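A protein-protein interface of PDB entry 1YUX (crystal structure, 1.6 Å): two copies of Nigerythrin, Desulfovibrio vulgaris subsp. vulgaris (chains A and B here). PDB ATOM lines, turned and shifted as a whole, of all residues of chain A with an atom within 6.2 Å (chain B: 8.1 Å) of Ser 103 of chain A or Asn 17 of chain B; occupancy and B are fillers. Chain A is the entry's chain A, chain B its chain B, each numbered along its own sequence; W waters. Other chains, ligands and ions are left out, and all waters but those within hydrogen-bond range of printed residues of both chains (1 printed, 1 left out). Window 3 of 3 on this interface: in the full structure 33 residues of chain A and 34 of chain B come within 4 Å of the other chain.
Water W1 lies within hydrogen-bond range of the backbone carbonyl oxygen of Thr 14 of chain B and the side-chain carboxylate of Asp 105 of chain A.
No position is printed for both chains.
Of the 10 printed residues of chain A, 4 touch a printed residue of chain B. Hydrophobic or aromatic side chains of chain A within 4 Å of the printed part of chain B: Leu 106 and Tyr 160. Of the 21 printed residues of chain B, 8 touch a printed residue of chain A. Among the printed residues, 11 pairs touch across the chains. Among the printed residues, no Asp or Glu carboxylate lies within 4 Å of a Lys or Arg side-chain nitrogen of the other chain.
The side-chain amide nitrogen (ND2) of Asn 107 of chain A lies close to the backbone carbonyl oxygen (O) of Ser 103 of chain A, at 3.4 Å. The backbone carbonyl oxygen (O) of Asn 15 of chain B sits at hydrogen-bond distance from the side-chain amino group (NZ) of Lys 146 of chain B, at 2.8 Å. N of Val 19 of chain B sits at hydrogen-bond distance from O of Ser 120 of chain B (3.0 Å). O of Lys 146 of chain B is in hydrogen-bond range of OG1 of Thr 119 of chain B, 2.8 Å away.
OD1 of Asp 105 of chain A lies within hydrogen-bond range of ND2 of Asn 17 of chain B (2.8 Å). ND2 of Asn 15 of chain B lies within hydrogen-bond range of O of Tyr 160 of chain A (3.0 Å). The side-chain hydroxyl (OH) of Tyr 160 of chain A lies within hydrogen-bond range of the backbone carbonyl oxygen (O) of Thr 119 of chain B, at 3.4 Å. The side-chain amino group of Lys 146 of chain B sits at hydrogen-bond distance from the side-chain hydroxyl of Tyr 160 of chain A (2.9 Å).
Ala 101 of chain A touches none of the printed residues of chain B. Of the printed residues of chain B, Ser 103 of chain A touches Asn 17 (3.5 Å). Of the printed residues of chain A, Asn 15 of chain B touches Asp 105 and Tyr 160. Printed residues of chain A within 4 Å of Asn 17 of chain B: Ser 103, Asp 105 and Leu 106. Of the printed residues of chain A, Val 19 of chain B touches Leu 106. Printed residues of chain A within 4 Å of Thr 119 of chain B: Tyr 160. Ser 120 of chain B touches none of the printed residues of chain A. Printed residues of chain A within 4 Å of Lys 146 of chain B: Tyr 160 (2.9 Å). The nearest printed residue of chain A that does not touch Asn 17 of chain B is Tyr 160 of chain A (4.9 Å).
Asn 17 of chain B touches Ser 103 of chain A (ND2 to CB, 3.5 Å). Asp 105 of chain A touches Thr 14 of chain B (CG to O, 3.3 Å). Asp 105 of chain A touches Asn 15 of chain B. N of Phe 16 of chain B touches OD2 of Asp 105 of chain A, at 3.6 Å. Leu 106 of chain A touches Asn 17 of chain B (CD2 to O, 3.6 Å). Leu 106 of chain A touches Met 18 of chain B (CD1 to O, 3.6 Å). Val 19 of chain B touches Leu 106 of chain A (N to CD2, 3.7 Å).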
ATOM      1  N   GLN A  57     -10.614   4.579 -29.857  1.00  0.00           N
ATOM      2  CA  GLN A  57     -11.058   5.678 -29.016  1.00  0.00           C
ATOM      3  C   GLN A  57     -10.752   7.039 -29.642  1.00  0.00           C
ATOM      4  O   GLN A  57     -11.131   8.076 -29.104  1.00  0.00           O
ATOM      5  CB  GLN A  57     -10.414   5.541 -27.634  1.00  0.00           C
ATOM      6  CG  GLN A  57     -10.787   4.217 -26.971  1.00  0.00           C
ATOM      7  CD  GLN A  57      -9.831   3.802 -25.871  1.00  0.00           C
ATOM      8  OE1 GLN A  57      -8.647   4.144 -25.898  1.00  0.00           O
ATOM      9  NE2 GLN A  57     -10.333   3.035 -24.911  1.00  0.00           N
ATOM     10  N   ALA A 101      -8.439  -4.072 -21.877  1.00  0.00           N
ATOM     11  CA  ALA A 101      -8.151  -2.673 -22.166  1.00  0.00           C
ATOM     12  C   ALA A 101      -9.313  -1.848 -21.644  1.00  0.00           C
ATOM     13  O   ALA A 101     -10.456  -2.305 -21.634  1.00  0.00           O
ATOM     14  CB  ALA A 101      -7.987  -2.456 -23.661  1.00  0.00           C
ATOM     15  N   TYR A 102      -9.014  -0.634 -21.202  1.00  0.00           N
ATOM     16  CA  TYR A 102     -10.032   0.262 -20.680  1.00  0.00           C
ATOM     17  C   TYR A 102      -9.931   1.570 -21.439  1.00  0.00           C
ATOM     18  O   TYR A 102      -9.415   1.595 -22.553  1.00  0.00           O
ATOM     19  CB  TYR A 102      -9.808   0.467 -19.179  1.00  0.00           C
ATOM     20  CG  TYR A 102      -9.925  -0.826 -18.408  1.00  0.00           C
ATOM     21  CD1 TYR A 102      -8.831  -1.680 -18.267  1.00  0.00           C
ATOM     22  CD2 TYR A 102     -11.150  -1.230 -17.877  1.00  0.00           C
ATOM     23  CE1 TYR A 102      -8.959  -2.910 -17.618  1.00  0.00           C
ATOM     24  CE2 TYR A 102     -11.288  -2.451 -17.231  1.00  0.00           C
ATOM     25  CZ  TYR A 102     -10.193  -3.286 -17.105  1.00  0.00           C
ATOM     26  OH  TYR A 102     -10.334  -4.499 -16.470  1.00  0.00           O
ATOM     27  N   SER A 103     -10.426   2.653 -20.851  1.00  0.00           N
ATOM     28  CA  SER A 103     -10.353   3.952 -21.508  1.00  0.00           C
ATOM     29  C   SER A 103      -8.893   4.335 -21.703  1.00  0.00           C
ATOM     30  O   SER A 103      -8.026   3.926 -20.928  1.00  0.00           O
ATOM     31  CB  SER A 103     -11.070   5.015 -20.677  1.00  0.00           C
ATOM     32  OG  SER A 103     -12.473   4.824 -20.726  1.00  0.00           O
ATOM     33  N   CYS A 104      -8.626   5.116 -22.743  1.00  0.00           N
ATOM     34  CA  CYS A 104      -7.268   5.533 -23.044  1.00  0.00           C
ATOM     35  C   CYS A 104      -6.510   6.129 -21.863  1.00  0.00           C
ATOM     36  O   CYS A 104      -5.364   5.754 -21.602  1.00  0.00           O
ATOM     37  CB  CYS A 104      -7.269   6.527 -24.200  1.00  0.00           C
ATOM     38  SG  CYS A 104      -5.614   6.850 -24.817  1.00  0.00           S
ATOM     39  N   ASP A 105      -7.138   7.056 -21.151  1.00  0.00           N
ATOM     40  CA  ASP A 105      -6.459   7.674 -20.019  1.00  0.00           C
ATOM     41  C   ASP A 105      -6.083   6.638 -18.962  1.00  0.00           C
ATOM     42  O   ASP A 105      -4.978   6.672 -18.416  1.00  0.00           O
ATOM     43  CB  ASP A 105      -7.316   8.812 -19.421  1.00  0.00           C
ATOM     44  CG  ASP A 105      -8.631   8.332 -18.833  1.00  0.00           C
ATOM     45  OD1 ASP A 105      -9.304   7.495 -19.466  1.00  0.00           O
ATOM     46  OD2 ASP A 105      -8.999   8.815 -17.741  1.00  0.00           O
ATOM     47  N   LEU A 106      -6.982   5.700 -18.690  1.00  0.00           N
ATOM     48  CA  LEU A 106      -6.696   4.669 -17.702  1.00  0.00           C
ATOM     49  C   LEU A 106      -5.593   3.729 -18.173  1.00  0.00           C
ATOM     50  O   LEU A 106      -4.802   3.242 -17.363  1.00  0.00           O
ATOM     51  CB  LEU A 106      -7.961   3.877 -17.378  1.00  0.00           C
ATOM     52  CG  LEU A 106      -9.007   4.697 -16.617  1.00  0.00           C
ATOM     53  CD1 LEU A 106     -10.232   3.844 -16.361  1.00  0.00           C
ATOM     54  CD2 LEU A 106      -8.420   5.191 -15.302  1.00  0.00           C
ATOM     55  N   ASN A 107      -5.536   3.474 -19.477  1.00  0.00           N
ATOM     56  CA  ASN A 107      -4.502   2.598 -20.014  1.00  0.00           C
ATOM     57  C   ASN A 107      -3.136   3.265 -19.884  1.00  0.00           C
ATOM     58  O   ASN A 107      -2.135   2.594 -19.637  1.00  0.00           O
ATOM     59  CB  ASN A 107      -4.781   2.254 -21.478  1.00  0.00           C
ATOM     60  CG  ASN A 107      -6.045   1.441 -21.650  1.00  0.00           C
ATOM     61  OD1 ASN A 107      -6.475   0.737 -20.734  1.00  0.00           O
ATOM     62  ND2 ASN A 107      -6.643   1.518 -22.832  1.00  0.00           N
ATOM     63  N   LEU A 108      -3.095   4.584 -20.052  1.00  0.00           N
ATOM     64  CA  LEU A 108      -1.839   5.312 -19.915  1.00  0.00           C
ATOM     65  C   LEU A 108      -1.357   5.207 -18.478  1.00  0.00           C
ATOM     66  O   LEU A 108      -0.166   5.038 -18.227  1.00  0.00           O
ATOM     67  CB  LEU A 108      -2.021   6.783 -20.294  1.00  0.00           C
ATOM     68  CG  LEU A 108      -2.114   7.060 -21.793  1.00  0.00           C
ATOM     69  CD1 LEU A 108      -2.583   8.492 -22.023  1.00  0.00           C
ATOM     70  CD2 LEU A 108      -0.745   6.828 -22.444  1.00  0.00           C
ATOM     71  N   TYR A 160      -0.772  11.443 -20.959  1.00  0.00           N
ATOM     72  CA  TYR A 160      -1.955  11.550 -20.119  1.00  0.00           C
ATOM     73  C   TYR A 160      -2.272  13.025 -19.861  1.00  0.00           C
ATOM     74  O   TYR A 160      -3.416  13.461 -19.977  1.00  0.00           O
ATOM     75  CB  TYR A 160      -1.690  10.831 -18.797  1.00  0.00           C
ATOM     76  CG  TYR A 160      -2.830  10.818 -17.807  1.00  0.00           C
ATOM     77  CD1 TYR A 160      -3.775   9.786 -17.808  1.00  0.00           C
ATOM     78  CD2 TYR A 160      -2.922  11.796 -16.818  1.00  0.00           C
ATOM     79  CE1 TYR A 160      -4.775   9.728 -16.834  1.00  0.00           C
ATOM     80  CE2 TYR A 160      -3.912  11.749 -15.846  1.00  0.00           C
ATOM     81  CZ  TYR A 160      -4.830  10.711 -15.855  1.00  0.00           C
ATOM     82  OH  TYR A 160      -5.768  10.640 -14.849  1.00  0.00           O
ATOM     83  N   VAL B  10     -14.086  18.474 -16.295  1.00  0.00           N
ATOM     84  CA  VAL B  10     -14.567  17.120 -16.490  1.00  0.00           C
ATOM     85  C   VAL B  10     -15.475  17.081 -17.724  1.00  0.00           C
ATOM     86  O   VAL B  10     -15.738  16.016 -18.280  1.00  0.00           O
ATOM     87  CB  VAL B  10     -15.342  16.627 -15.244  1.00  0.00           C
ATOM     88  CG1 VAL B  10     -16.622  17.427 -15.074  1.00  0.00           C
ATOM     89  CG2 VAL B  10     -15.632  15.143 -15.362  1.00  0.00           C
ATOM     90  N   ALA B  13     -12.551  17.432 -20.920  1.00  0.00           N
ATOM     91  CA  ALA B  13     -11.319  16.653 -20.843  1.00  0.00           C
ATOM     92  C   ALA B  13     -11.630  15.167 -20.796  1.00  0.00           C
ATOM     93  O   ALA B  13     -12.723  14.767 -20.386  1.00  0.00           O
ATOM     94  CB  ALA B  13     -10.518  17.063 -19.619  1.00  0.00           C
ATOM     95  N   THR B  14     -10.666  14.343 -21.199  1.00  0.00           N
ATOM     96  CA  THR B  14     -10.882  12.905 -21.225  1.00  0.00           C
ATOM     97  C   THR B  14      -9.942  12.066 -20.367  1.00  0.00           C
ATOM     98  O   THR B  14      -9.795  10.863 -20.593  1.00  0.00           O
ATOM     99  CB  THR B  14     -10.850  12.372 -22.671  1.00  0.00           C
ATOM    100  OG1 THR B  14      -9.563  12.613 -23.255  1.00  0.00           O
ATOM    101  CG2 THR B  14     -11.925  13.065 -23.504  1.00  0.00           C
ATOM    102  N   ASN B  15      -9.301  12.691 -19.386  1.00  0.00           N
ATOM    103  CA  ASN B  15      -8.430  11.946 -18.492  1.00  0.00           C
ATOM    104  C   ASN B  15      -8.957  12.048 -17.064  1.00  0.00           C
ATOM    105  O   ASN B  15      -8.193  12.113 -16.104  1.00  0.00           O
ATOM    106  CB  ASN B  15      -6.975  12.443 -18.582  1.00  0.00           C
ATOM    107  CG  ASN B  15      -6.826  13.918 -18.274  1.00  0.00           C
ATOM    108  OD1 ASN B  15      -7.807  14.645 -18.126  1.00  0.00           O
ATOM    109  ND2 ASN B  15      -5.577  14.371 -18.181  1.00  0.00           N
ATOM    110  N   PHE B  16     -10.281  12.038 -16.935  1.00  0.00           N
ATOM    111  CA  PHE B  16     -10.923  12.134 -15.629  1.00  0.00           C
ATOM    112  C   PHE B  16     -11.527  10.833 -15.121  1.00  0.00           C
ATOM    113  O   PHE B  16     -12.223  10.822 -14.104  1.00  0.00           O
ATOM    114  CB  PHE B  16     -12.001  13.223 -15.651  1.00  0.00           C
ATOM    115  CG  PHE B  16     -11.453  14.611 -15.492  1.00  0.00           C
ATOM    116  CD1 PHE B  16     -10.674  15.186 -16.490  1.00  0.00           C
ATOM    117  CD2 PHE B  16     -11.685  15.329 -14.325  1.00  0.00           C
ATOM    118  CE1 PHE B  16     -10.130  16.461 -16.327  1.00  0.00           C
ATOM    119  CE2 PHE B  16     -11.144  16.608 -14.151  1.00  0.00           C
ATOM    120  CZ  PHE B  16     -10.366  17.171 -15.154  1.00  0.00           C
ATOM    121  N   ASN B  17     -11.263   9.732 -15.813  1.00  0.00           N
ATOM    122  CA  ASN B  17     -11.807   8.457 -15.377  1.00  0.00           C
ATOM    123  C   ASN B  17     -11.094   7.948 -14.134  1.00  0.00           C
ATOM    124  O   ASN B  17      -9.912   8.218 -13.918  1.00  0.00           O
ATOM    125  CB  ASN B  17     -11.712   7.420 -16.497  1.00  0.00           C
ATOM    126  CG  ASN B  17     -12.614   7.754 -17.666  1.00  0.00           C
ATOM    127  OD1 ASN B  17     -13.827   7.897 -17.502  1.00  0.00           O
ATOM    128  ND2 ASN B  17     -12.028   7.889 -18.852  1.00  0.00           N
ATOM    129  N   MET B  18     -11.841   7.227 -13.308  1.00  0.00           N
ATOM    130  CA  MET B  18     -11.316   6.644 -12.082  1.00  0.00           C
ATOM    131  C   MET B  18     -10.943   5.195 -12.383  1.00  0.00           C
ATOM    132  O   MET B  18     -11.683   4.500 -13.077  1.00  0.00           O
ATOM    133  CB  MET B  18     -12.390   6.671 -10.996  1.00  0.00           C
ATOM    134  CG  MET B  18     -11.988   5.974  -9.712  1.00  0.00           C
ATOM    135  SD  MET B  18     -13.415   5.616  -8.674  1.00  0.00           S
ATOM    136  CE  MET B  18     -14.020   4.127  -9.467  1.00  0.00           C
ATOM    137  N   VAL B  19      -9.798   4.745 -11.882  1.00  0.00           N
ATOM    138  CA  VAL B  19      -9.384   3.365 -12.101  1.00  0.00           C
ATOM    139  C   VAL B  19     -10.517   2.495 -11.559  1.00  0.00           C
ATOM    140  O   VAL B  19     -11.033   2.746 -10.467  1.00  0.00           O
ATOM    141  CB  VAL B  19      -8.062   3.049 -11.360  1.00  0.00           C
ATOM    142  CG1 VAL B  19      -6.947   3.929 -11.899  1.00  0.00           C
ATOM    143  CG2 VAL B  19      -8.224   3.271  -9.863  1.00  0.00           C
ATOM    144  N   ALA B  20     -10.915   1.484 -12.326  1.00  0.00           N
ATOM    145  CA  ALA B  20     -12.009   0.611 -11.917  1.00  0.00           C
ATOM    146  C   ALA B  20     -11.777  -0.026 -10.555  1.00  0.00           C
ATOM    147  O   ALA B  20     -12.693  -0.102  -9.735  1.00  0.00           O
ATOM    148  CB  ALA B  20     -12.236  -0.464 -12.967  1.00  0.00           C
ATOM    149  N   ILE B 116       0.038   9.726  -8.876  1.00  0.00           N
ATOM    150  CA  ILE B 116      -0.758   8.939  -9.801  1.00  0.00           C
ATOM    151  C   ILE B 116      -2.034   8.460  -9.115  1.00  0.00           C
ATOM    152  O   ILE B 116      -3.117   8.495  -9.705  1.00  0.00           O
ATOM    153  CB  ILE B 116       0.052   7.746 -10.330  1.00  0.00           C
ATOM    154  CG1 ILE B 116       1.151   8.266 -11.264  1.00  0.00           C
ATOM    155  CG2 ILE B 116      -0.867   6.767 -11.051  1.00  0.00           C
ATOM    156  CD1 ILE B 116       2.163   7.220 -11.681  1.00  0.00           C
ATOM    157  N   GLU B 118      -3.598   9.865  -6.654  1.00  0.00           N
ATOM    158  CA  GLU B 118      -4.495  11.002  -6.499  1.00  0.00           C
ATOM    159  C   GLU B 118      -5.161  11.447  -7.796  1.00  0.00           C
ATOM    160  O   GLU B 118      -6.353  11.757  -7.808  1.00  0.00           O
ATOM    161  CB  GLU B 118      -3.746  12.178  -5.858  1.00  0.00           C
ATOM    162  CG  GLU B 118      -3.227  11.857  -4.463  1.00  0.00           C
ATOM    163  CD  GLU B 118      -2.439  12.993  -3.832  1.00  0.00           C
ATOM    164  OE1 GLU B 118      -3.030  14.055  -3.552  1.00  0.00           O
ATOM    165  OE2 GLU B 118      -1.224  12.818  -3.610  1.00  0.00           O
ATOM    166  N   THR B 119      -4.399  11.488  -8.885  1.00  0.00           N
ATOM    167  CA  THR B 119      -4.942  11.946 -10.157  1.00  0.00           C
ATOM    168  C   THR B 119      -5.829  10.950 -10.889  1.00  0.00           C
ATOM    169  O   THR B 119      -6.730  11.348 -11.630  1.00  0.00           O
ATOM    170  CB  THR B 119      -3.816  12.376 -11.130  1.00  0.00           C
ATOM    171  OG1 THR B 119      -4.348  13.292 -12.093  1.00  0.00           O
ATOM    172  CG2 THR B 119      -3.244  11.162 -11.874  1.00  0.00           C
ATOM    173  N   SER B 120      -5.591   9.660 -10.681  1.00  0.00           N
ATOM    174  CA  SER B 120      -6.354   8.637 -11.388  1.00  0.00           C
ATOM    175  C   SER B 120      -7.308   7.831 -10.527  1.00  0.00           C
ATOM    176  O   SER B 120      -8.098   7.042 -11.048  1.00  0.00           O
ATOM    177  CB  SER B 120      -5.398   7.660 -12.073  1.00  0.00           C
ATOM    178  OG  SER B 120      -4.695   6.893 -11.106  1.00  0.00           O
ATOM    179  N   ASP B 121      -7.236   8.023  -9.218  1.00  0.00           N
ATOM    180  CA  ASP B 121      -8.077   7.260  -8.316  1.00  0.00           C
ATOM    181  C   ASP B 121      -8.863   8.137  -7.348  1.00  0.00           C
ATOM    182  O   ASP B 121     -10.074   8.295  -7.490  1.00  0.00           O
ATOM    183  CB  ASP B 121      -7.204   6.265  -7.539  1.00  0.00           C
ATOM    184  CG  ASP B 121      -8.015   5.286  -6.719  1.00  0.00           C
ATOM    185  OD1 ASP B 121      -9.103   5.674  -6.252  1.00  0.00           O
ATOM    186  OD2 ASP B 121      -7.554   4.139  -6.529  1.00  0.00           O
ATOM    187  N   MET B 122      -8.171   8.722  -6.376  1.00  0.00           N
ATOM    188  CA  MET B 122      -8.837   9.532  -5.367  1.00  0.00           C
ATOM    189  C   MET B 122      -9.641  10.715  -5.883  1.00  0.00           C
ATOM    190  O   MET B 122     -10.851  10.789  -5.663  1.00  0.00           O
ATOM    191  CB  MET B 122      -7.832  10.034  -4.336  1.00  0.00           C
ATOM    192  CG  MET B 122      -8.500  10.730  -3.165  1.00  0.00           C
ATOM    193  SD  MET B 122      -7.337  11.509  -2.058  1.00  0.00           S
ATOM    194  CE  MET B 122      -7.061  13.040  -2.928  1.00  0.00           C
ATOM    195  N   TYR B 123      -8.988  11.655  -6.555  1.00  0.00           N
ATOM    196  CA  TYR B 123      -9.738  12.804  -7.036  1.00  0.00           C
ATOM    197  C   TYR B 123     -10.823  12.429  -8.040  1.00  0.00           C
ATOM    198  O   TYR B 123     -11.926  12.964  -7.969  1.00  0.00           O
ATOM    199  CB  TYR B 123      -8.790  13.886  -7.564  1.00  0.00           C
ATOM    200  CG  TYR B 123      -8.181  14.690  -6.430  1.00  0.00           C
ATOM    201  CD1 TYR B 123      -6.799  14.810  -6.288  1.00  0.00           C
ATOM    202  CD2 TYR B 123      -8.998  15.313  -5.481  1.00  0.00           C
ATOM    203  CE1 TYR B 123      -6.240  15.532  -5.224  1.00  0.00           C
ATOM    204  CE2 TYR B 123      -8.454  16.034  -4.417  1.00  0.00           C
ATOM    205  CZ  TYR B 123      -7.077  16.140  -4.294  1.00  0.00           C
ATOM    206  OH  TYR B 123      -6.551  16.850  -3.241  1.00  0.00           O
ATOM    207  N   PRO B 124     -10.541  11.508  -8.979  1.00  0.00           N
ATOM    208  CA  PRO B 124     -11.615  11.162  -9.916  1.00  0.00           C
ATOM    209  C   PRO B 124     -12.822  10.589  -9.164  1.00  0.00           C
ATOM    210  O   PRO B 124     -13.966  10.845  -9.530  1.00  0.00           O
ATOM    211  CB  PRO B 124     -10.961  10.130 -10.823  1.00  0.00           C
ATOM    212  CG  PRO B 124      -9.562  10.636 -10.916  1.00  0.00           C
ATOM    213  CD  PRO B 124      -9.246  11.000  -9.470  1.00  0.00           C
ATOM    214  N   ALA B 125     -12.561   9.821  -8.109  1.00  0.00           N
ATOM    215  CA  ALA B 125     -13.641   9.229  -7.317  1.00  0.00           C
ATOM    216  C   ALA B 125     -14.439  10.322  -6.623  1.00  0.00           C
ATOM    217  O   ALA B 125     -15.676  10.301  -6.614  1.00  0.00           O
ATOM    218  CB  ALA B 125     -13.070   8.267  -6.282  1.00  0.00           C
ATOM    219  N   ILE B 127     -14.549  13.472  -7.507  1.00  0.00           N
ATOM    220  CA  ILE B 127     -15.187  14.301  -8.522  1.00  0.00           C
ATOM    221  C   ILE B 127     -16.515  13.668  -8.930  1.00  0.00           C
ATOM    222  O   ILE B 127     -17.539  14.347  -8.990  1.00  0.00           O
ATOM    223  CB  ILE B 127     -14.284  14.459  -9.768  1.00  0.00           C
ATOM    224  CG1 ILE B 127     -13.069  15.325  -9.411  1.00  0.00           C
ATOM    225  CG2 ILE B 127     -15.071  15.087 -10.914  1.00  0.00           C
ATOM    226  CD1 ILE B 127     -12.018  15.400 -10.495  1.00  0.00           C
ATOM    227  N   ARG B 128     -16.493  12.365  -9.196  1.00  0.00           N
ATOM    228  CA  ARG B 128     -17.703  11.648  -9.586  1.00  0.00           C
ATOM    229  C   ARG B 128     -18.788  11.796  -8.532  1.00  0.00           C
ATOM    230  O   ARG B 128     -19.949  12.031  -8.859  1.00  0.00           O
ATOM    231  CB  ARG B 128     -17.409  10.158  -9.796  1.00  0.00           C
ATOM    232  CG  ARG B 128     -16.605   9.857 -11.040  1.00  0.00           C
ATOM    233  CD  ARG B 128     -16.442   8.362 -11.253  1.00  0.00           C
ATOM    234  NE  ARG B 128     -15.718   8.081 -12.489  1.00  0.00           N
ATOM    235  CZ  ARG B 128     -15.540   6.866 -13.001  1.00  0.00           C
ATOM    236  NH1 ARG B 128     -16.039   5.795 -12.386  1.00  0.00           N
ATOM    237  NH2 ARG B 128     -14.855   6.724 -14.132  1.00  0.00           N
ATOM    238  N   LYS B 146      -6.904  17.574  -9.044  1.00  0.00           N
ATOM    239  CA  LYS B 146      -6.670  16.407  -9.890  1.00  0.00           C
ATOM    240  C   LYS B 146      -5.725  16.700 -11.053  1.00  0.00           C
ATOM    241  O   LYS B 146      -4.791  15.937 -11.312  1.00  0.00           O
ATOM    242  CB  LYS B 146      -8.013  15.878 -10.415  1.00  0.00           C
ATOM    243  CG  LYS B 146      -7.933  14.708 -11.397  1.00  0.00           C
ATOM    244  CD  LYS B 146      -7.811  15.181 -12.840  1.00  0.00           C
ATOM    245  CE  LYS B 146      -7.967  14.038 -13.837  1.00  0.00           C
ATOM    246  NZ  LYS B 146      -6.817  13.087 -13.829  1.00  0.00           N
HETATM  247  O   HOH W   1      -9.747   8.652 -22.358  1.00  0.00           O
